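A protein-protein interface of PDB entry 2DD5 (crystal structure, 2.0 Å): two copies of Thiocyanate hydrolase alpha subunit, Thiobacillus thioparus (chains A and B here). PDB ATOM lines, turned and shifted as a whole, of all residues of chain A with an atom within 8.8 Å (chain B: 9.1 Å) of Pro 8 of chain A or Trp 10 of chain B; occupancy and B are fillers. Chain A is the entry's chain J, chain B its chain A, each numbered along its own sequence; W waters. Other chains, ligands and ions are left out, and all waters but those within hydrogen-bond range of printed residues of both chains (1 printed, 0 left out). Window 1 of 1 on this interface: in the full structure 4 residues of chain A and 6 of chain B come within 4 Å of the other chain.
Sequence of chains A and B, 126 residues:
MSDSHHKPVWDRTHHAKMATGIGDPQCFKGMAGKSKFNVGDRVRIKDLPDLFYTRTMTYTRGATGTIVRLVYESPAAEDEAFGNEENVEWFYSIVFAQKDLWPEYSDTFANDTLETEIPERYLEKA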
ATOM      1  N   LYS A   7     -29.124  21.255  21.370  1.00  0.00           N
ATOM      2  CA  LYS A   7     -27.794  20.602  21.560  1.00  0.00           C
ATOM      3  C   LYS A   7     -26.641  21.505  21.138  1.00  0.00           C
ATOM      4  O   LYS A   7     -26.772  22.314  20.220  1.00  0.00           O
ATOM      5  CB  LYS A   7     -27.724  19.293  20.775  1.00  0.00           C
ATOM      6  CG  LYS A   7     -28.555  18.169  21.368  1.00  0.00           C
ATOM      7  CD  LYS A   7     -28.325  16.877  20.604  1.00  0.00           C
ATOM      8  CE  LYS A   7     -29.088  15.721  21.221  1.00  0.00           C
ATOM      9  NZ  LYS A   7     -28.931  14.476  20.414  1.00  0.00           N
ATOM     10  N   PRO A   8     -25.486  21.365  21.807  1.00  0.00           N
ATOM     11  CA  PRO A   8     -24.286  22.158  21.527  1.00  0.00           C
ATOM     12  C   PRO A   8     -23.727  21.958  20.124  1.00  0.00           C
ATOM     13  O   PRO A   8     -23.836  20.879  19.545  1.00  0.00           O
ATOM     14  CB  PRO A   8     -23.301  21.684  22.595  1.00  0.00           C
ATOM     15  CG  PRO A   8     -24.188  21.238  23.706  1.00  0.00           C
ATOM     16  CD  PRO A   8     -25.266  20.494  22.973  1.00  0.00           C
ATOM     17  N   VAL A   9     -23.127  23.012  19.587  1.00  0.00           N
ATOM     18  CA  VAL A   9     -22.515  22.951  18.271  1.00  0.00           C
ATOM     19  C   VAL A   9     -21.020  23.162  18.472  1.00  0.00           C
ATOM     20  O   VAL A   9     -20.610  24.082  19.182  1.00  0.00           O
ATOM     21  CB  VAL A   9     -23.051  24.056  17.336  1.00  0.00           C
ATOM     22  CG1 VAL A   9     -22.349  23.977  15.991  1.00  0.00           C
ATOM     23  CG2 VAL A   9     -24.552  23.904  17.152  1.00  0.00           C
ATOM     24  N   TRP A  10     -20.208  22.304  17.863  1.00  0.00           N
ATOM     25  CA  TRP A  10     -18.761  22.418  17.990  1.00  0.00           C
ATOM     26  C   TRP A  10     -18.148  22.940  16.702  1.00  0.00           C
ATOM     27  O   TRP A  10     -18.323  22.350  15.635  1.00  0.00           O
ATOM     28  CB  TRP A  10     -18.144  21.063  18.337  1.00  0.00           C
ATOM     29  CG  TRP A  10     -18.783  20.420  19.516  1.00  0.00           C
ATOM     30  CD1 TRP A  10     -19.923  19.668  19.521  1.00  0.00           C
ATOM     31  CD2 TRP A  10     -18.360  20.517  20.877  1.00  0.00           C
ATOM     32  NE1 TRP A  10     -20.236  19.293  20.804  1.00  0.00           N
ATOM     33  CE2 TRP A  10     -19.294  19.801  21.658  1.00  0.00           C
ATOM     34  CE3 TRP A  10     -17.281  21.143  21.517  1.00  0.00           C
ATOM     35  CZ2 TRP A  10     -19.184  19.692  23.045  1.00  0.00           C
ATOM     36  CZ3 TRP A  10     -17.171  21.034  22.898  1.00  0.00           C
ATOM     37  CH2 TRP A  10     -18.118  20.313  23.647  1.00  0.00           C
ATOM     38  N   ASP A  11     -17.435  24.055  16.811  1.00  0.00           N
ATOM     39  CA  ASP A  11     -16.781  24.669  15.665  1.00  0.00           C
ATOM     40  C   ASP A  11     -15.604  23.787  15.264  1.00  0.00           C
ATOM     41  O   ASP A  11     -14.553  23.817  15.905  1.00  0.00           O
ATOM     42  CB  ASP A  11     -16.278  26.059  16.048  1.00  0.00           C
ATOM     43  CG  ASP A  11     -15.604  26.769  14.897  1.00  0.00           C
ATOM     44  OD1 ASP A  11     -14.832  26.115  14.165  1.00  0.00           O
ATOM     45  OD2 ASP A  11     -15.836  27.982  14.735  1.00  0.00           O
ATOM     46  N   PHE A  82      -9.430  21.031  27.515  1.00  0.00           N
ATOM     47  CA  PHE A  82     -10.858  21.181  27.773  1.00  0.00           C
ATOM     48  C   PHE A  82     -11.530  22.150  26.806  1.00  0.00           C
ATOM     49  O   PHE A  82     -12.635  22.641  27.062  1.00  0.00           O
ATOM     50  CB  PHE A  82     -11.085  21.599  29.228  1.00  0.00           C
ATOM     51  CG  PHE A  82     -10.887  20.470  30.205  1.00  0.00           C
ATOM     52  CD1 PHE A  82     -11.894  19.534  30.420  1.00  0.00           C
ATOM     53  CD2 PHE A  82      -9.669  20.303  30.855  1.00  0.00           C
ATOM     54  CE1 PHE A  82     -11.690  18.443  31.267  1.00  0.00           C
ATOM     55  CE2 PHE A  82      -9.454  19.217  31.701  1.00  0.00           C
ATOM     56  CZ  PHE A  82     -10.463  18.286  31.908  1.00  0.00           C
ATOM     57  N   PRO B   8     -19.212  26.479  22.493  1.00  0.00           N
ATOM     58  CA  PRO B   8     -20.292  25.479  22.691  1.00  0.00           C
ATOM     59  C   PRO B   8     -21.264  25.981  23.753  1.00  0.00           C
ATOM     60  O   PRO B   8     -20.857  26.306  24.866  1.00  0.00           O
ATOM     61  CB  PRO B   8     -19.631  24.185  23.148  1.00  0.00           C
ATOM     62  CG  PRO B   8     -18.190  24.378  22.652  1.00  0.00           C
ATOM     63  CD  PRO B   8     -17.910  25.876  22.826  1.00  0.00           C
ATOM     64  N   VAL B   9     -22.546  26.047  23.413  1.00  0.00           N
ATOM     65  CA  VAL B   9     -23.534  26.509  24.375  1.00  0.00           C
ATOM     66  C   VAL B   9     -24.448  25.366  24.802  1.00  0.00           C
ATOM     67  O   VAL B   9     -25.061  24.692  23.972  1.00  0.00           O
ATOM     68  CB  VAL B   9     -24.395  27.668  23.806  1.00  0.00           C
ATOM     69  CG1 VAL B   9     -23.492  28.737  23.209  1.00  0.00           C
ATOM     70  CG2 VAL B   9     -25.374  27.149  22.769  1.00  0.00           C
ATOM     71  N   TRP B  10     -24.513  25.137  26.107  1.00  0.00           N
ATOM     72  CA  TRP B  10     -25.359  24.088  26.643  1.00  0.00           C
ATOM     73  C   TRP B  10     -26.651  24.727  27.128  1.00  0.00           C
ATOM     74  O   TRP B  10     -26.635  25.651  27.944  1.00  0.00           O
ATOM     75  CB  TRP B  10     -24.653  23.364  27.792  1.00  0.00           C
ATOM     76  CG  TRP B  10     -23.363  22.717  27.378  1.00  0.00           C
ATOM     77  CD1 TRP B  10     -22.145  23.323  27.245  1.00  0.00           C
ATOM     78  CD2 TRP B  10     -23.175  21.350  26.994  1.00  0.00           C
ATOM     79  NE1 TRP B  10     -21.211  22.417  26.800  1.00  0.00           N
ATOM     80  CE2 TRP B  10     -21.816  21.199  26.638  1.00  0.00           C
ATOM     81  CE3 TRP B  10     -24.023  20.236  26.916  1.00  0.00           C
ATOM     82  CZ2 TRP B  10     -21.284  19.979  26.207  1.00  0.00           C
ATOM     83  CZ3 TRP B  10     -23.494  19.020  26.488  1.00  0.00           C
ATOM     84  CH2 TRP B  10     -22.136  18.903  26.140  1.00  0.00           C
ATOM     85  N   ASP B  11     -27.766  24.238  26.603  1.00  0.00           N
ATOM     86  CA  ASP B  11     -29.080  24.752  26.954  1.00  0.00           C
ATOM     87  C   ASP B  11     -29.439  24.360  28.383  1.00  0.00           C
ATOM     88  O   ASP B  11     -29.693  23.190  28.660  1.00  0.00           O
ATOM     89  CB  ASP B  11     -30.115  24.178  25.992  1.00  0.00           C
ATOM     90  CG  ASP B  11     -31.440  24.888  26.074  1.00  0.00           C
ATOM     91  OD1 ASP B  11     -31.804  25.338  27.179  1.00  0.00           O
ATOM     92  OD2 ASP B  11     -32.120  24.987  25.032  1.00  0.00           O
ATOM     93  N   ARG B  12     -29.476  25.329  29.292  1.00  0.00           N
ATOM     94  CA  ARG B  12     -29.799  25.019  30.680  1.00  0.00           C
ATOM     95  C   ARG B  12     -31.268  25.244  31.035  1.00  0.00           C
ATOM     96  O   ARG B  12     -31.644  25.161  32.205  1.00  0.00           O
ATOM     97  CB  ARG B  12     -28.907  25.833  31.623  1.00  0.00           C
ATOM     98  CG  ARG B  12     -27.432  25.774  31.263  1.00  0.00           C
ATOM     99  CD  ARG B  12     -26.536  26.133  32.436  1.00  0.00           C
ATOM    100  NE  ARG B  12     -26.796  27.449  33.013  1.00  0.00           N
ATOM    101  CZ  ARG B  12     -26.475  28.608  32.450  1.00  0.00           C
ATOM    102  NH1 ARG B  12     -26.755  29.742  33.076  1.00  0.00           N
ATOM    103  NH2 ARG B  12     -25.877  28.643  31.270  1.00  0.00           N
ATOM    104  N   THR B  13     -32.100  25.525  30.033  1.00  0.00           N
ATOM    105  CA  THR B  13     -33.522  25.759  30.286  1.00  0.00           C
ATOM    106  C   THR B  13     -34.419  24.699  29.649  1.00  0.00           C
ATOM    107  O   THR B  13     -35.592  24.576  30.009  1.00  0.00           O
ATOM    108  CB  THR B  13     -33.981  27.139  29.754  1.00  0.00           C
ATOM    109  OG1 THR B  13     -33.785  27.196  28.335  1.00  0.00           O
ATOM    110  CG2 THR B  13     -33.201  28.260  30.423  1.00  0.00           C
ATOM    111  N   HIS B  14     -33.864  23.935  28.714  1.00  0.00           N
ATOM    112  CA  HIS B  14     -34.626  22.910  28.014  1.00  0.00           C
ATOM    113  C   HIS B  14     -35.434  21.957  28.893  1.00  0.00           C
ATOM    114  O   HIS B  14     -36.646  21.819  28.717  1.00  0.00           O
ATOM    115  CB  HIS B  14     -33.711  22.077  27.116  1.00  0.00           C
ATOM    116  CG  HIS B  14     -34.424  20.959  26.425  1.00  0.00           C
ATOM    117  ND1 HIS B  14     -35.424  21.177  25.503  1.00  0.00           N
ATOM    118  CD2 HIS B  14     -34.340  19.616  26.579  1.00  0.00           C
ATOM    119  CE1 HIS B  14     -35.929  20.017  25.121  1.00  0.00           C
ATOM    120  NE2 HIS B  14     -35.289  19.054  25.760  1.00  0.00           N
ATOM    121  N   GLU B  80     -30.191   9.513  27.359  1.00  0.00           N
ATOM    122  CA  GLU B  80     -30.371  10.615  28.291  1.00  0.00           C
ATOM    123  C   GLU B  80     -29.053  10.972  28.995  1.00  0.00           C
ATOM    124  O   GLU B  80     -28.743  12.147  29.202  1.00  0.00           O
ATOM    125  CB  GLU B  80     -31.439  10.223  29.319  1.00  0.00           C
ATOM    126  CG  GLU B  80     -32.045  11.368  30.100  1.00  0.00           C
ATOM    127  CD  GLU B  80     -33.269  10.926  30.891  1.00  0.00           C
ATOM    128  OE1 GLU B  80     -33.129  10.036  31.756  1.00  0.00           O
ATOM    129  OE2 GLU B  80     -34.370  11.466  30.646  1.00  0.00           O
ATOM    130  N   ALA B  81     -28.273   9.954  29.340  1.00  0.00           N
ATOM    131  CA  ALA B  81     -27.004  10.161  30.033  1.00  0.00           C
ATOM    132  C   ALA B  81     -25.977  10.940  29.218  1.00  0.00           C
ATOM    133  O   ALA B  81     -24.973  11.394  29.762  1.00  0.00           O
ATOM    134  CB  ALA B  81     -26.417   8.815  30.462  1.00  0.00           C
ATOM    135  N   PHE B  82     -26.223  11.084  27.917  1.00  0.00           N
ATOM    136  CA  PHE B  82     -25.314  11.819  27.044  1.00  0.00           C
ATOM    137  C   PHE B  82     -25.995  13.015  26.383  1.00  0.00           C
ATOM    138  O   PHE B  82     -25.515  13.542  25.380  1.00  0.00           O
ATOM    139  CB  PHE B  82     -24.722  10.877  25.989  1.00  0.00           C
ATOM    140  CG  PHE B  82     -23.705   9.920  26.550  1.00  0.00           C
ATOM    141  CD1 PHE B  82     -22.382  10.318  26.733  1.00  0.00           C
ATOM    142  CD2 PHE B  82     -24.082   8.642  26.951  1.00  0.00           C
ATOM    143  CE1 PHE B  82     -21.449   9.454  27.313  1.00  0.00           C
ATOM    144  CE2 PHE B  82     -23.160   7.771  27.532  1.00  0.00           C
ATOM    145  CZ  PHE B  82     -21.841   8.177  27.714  1.00  0.00           C
ATOM    146  N   GLY B  83     -27.119  13.432  26.959  1.00  0.00           N
ATOM    147  CA  GLY B  83     -27.845  14.585  26.453  1.00  0.00           C
ATOM    148  C   GLY B  83     -28.704  14.374  25.222  1.00  0.00           C
ATOM    149  O   GLY B  83     -29.128  15.344  24.596  1.00  0.00           O
ATOM    150  N   ASN B  84     -28.975  13.120  24.882  1.00  0.00           N
ATOM    151  CA  ASN B  84     -29.777  12.806  23.705  1.00  0.00           C
ATOM    152  C   ASN B  84     -31.181  12.376  24.127  1.00  0.00           C
ATOM    153  O   ASN B  84     -31.393  11.243  24.559  1.00  0.00           O
ATOM    154  CB  ASN B  84     -29.100  11.690  22.905  1.00  0.00           C
ATOM    155  CG  ASN B  84     -27.648  12.011  22.568  1.00  0.00           C
ATOM    156  OD1 ASN B  84     -26.738  11.218  22.838  1.00  0.00           O
ATOM    157  ND2 ASN B  84     -27.424  13.175  21.971  1.00  0.00           N
ATOM    158  N   GLU B  86     -34.012  13.052  22.015  1.00  0.00           N
ATOM    159  CA  GLU B  86     -34.862  13.083  20.827  1.00  0.00           C
ATOM    160  C   GLU B  86     -35.762  11.860  20.706  1.00  0.00           C
ATOM    161  O   GLU B  86     -36.890  11.963  20.226  1.00  0.00           O
ATOM    162  CB  GLU B  86     -34.016  13.176  19.552  1.00  0.00           C
ATOM    163  CG  GLU B  86     -32.795  14.068  19.660  1.00  0.00           C
ATOM    164  CD  GLU B  86     -31.719  13.460  20.543  1.00  0.00           C
ATOM    165  OE1 GLU B  86     -31.165  12.396  20.186  1.00  0.00           O
ATOM    166  OE2 GLU B  86     -31.435  14.050  21.602  1.00  0.00           O
HETATM  167  O   HOH W   1     -23.223  25.580  20.718  1.00  0.00           O
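Pro 8 of chain A touches Val 9 of chain B, and with the chains exchanged Val 9 of chain A touches Pro 8 of chain B.
Pro 8 of chain A touches Trp 10 of chain B, and with the chains exchanged Trp 10 of chain A touches Pro 8 of chain B.
Trp 10 of chain A touches its own counterpart, Trp 10 of chain B.
Of the 8 pairs that touch across the chains among the printed residues, 5 have their exchanged pair printed and touching as well.
Pro 8 of chain A touches two residues of chain B.
Of chain A, only Pro 8 (3.4 Å) and Trp 10 (3.8 Å) come within 4 Å of Trp 10 of chain B.
Of chain B, only Pro 8 comes within 4 Å of Val 9 of chain A.
Of chain A, only Pro 8 comes within 4 Å of Val 9 of chain B.
Of the printed residues of chain A, Gly 83 of chain B touches Lys 7.
Printed residues of chain A within 4 Å of Pro 8 of chain B: Val 9 and Trp 10.
Of the printed residues of chain B, Trp 10 of chain A touches Pro 8 and Trp 10.
Printed residues of chain A within 4 Å of Glu 86 of chain B: Lys 7 (2.8 Å).
Arg 12 of chain B touches none of the printed residues of chain A.
Ala 81 of chain B touches none of the printed residues of chain A.
The nearest residue of chain B that does not touch Pro 8 of chain A is Pro 8 of chain B (4.5 Å).
The nearest residue of chain A that does not touch Trp 10 of chain B is Lys 7 of chain A (6.2 Å).
Printed residues of chain A that touch a printed residue of chain B: Lys 7, Pro 8, Val 9 and Trp 10.
Hydrophobic or aromatic side chains of chain A that line the printed part of chain B: Pro 8 and Trp 10.
Of the 13 printed residues of chain B, 6 touch a printed residue of chain A.
Printed residues of chain B that touch a printed residue of chain A: Pro 8, Val 9, Trp 10, Gly 83, Asn 84 and Glu 86.
NZ of Lys 7 of chain A sits close to ND2 of Asn 84 of chain B (2.5 Å).
NZ of Lys 7 of chain A is in salt-bridge range of OE2 of Glu 86 of chain B, 2.8 Å away.
Water W1 bridges the backbone NH of Val 9 of chain A (2.8 Å) and the backbone NH of Val 9 of chain B (2.8 Å).
Lys 7 of chain A touches Gly 83 of chain B.
Val 9 of chain B touches Pro 8 of chain A.
Pro 8 of chain A touches Trp 10 of chain B.
Val 9 of chain A touches Pro 8 of chain B.
Pro 8 of chain B touches Trp 10 of chain A.
Trp 10 of chain B touches Trp 10 of chain A (CZ2 to CZ2, 3.8 Å).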
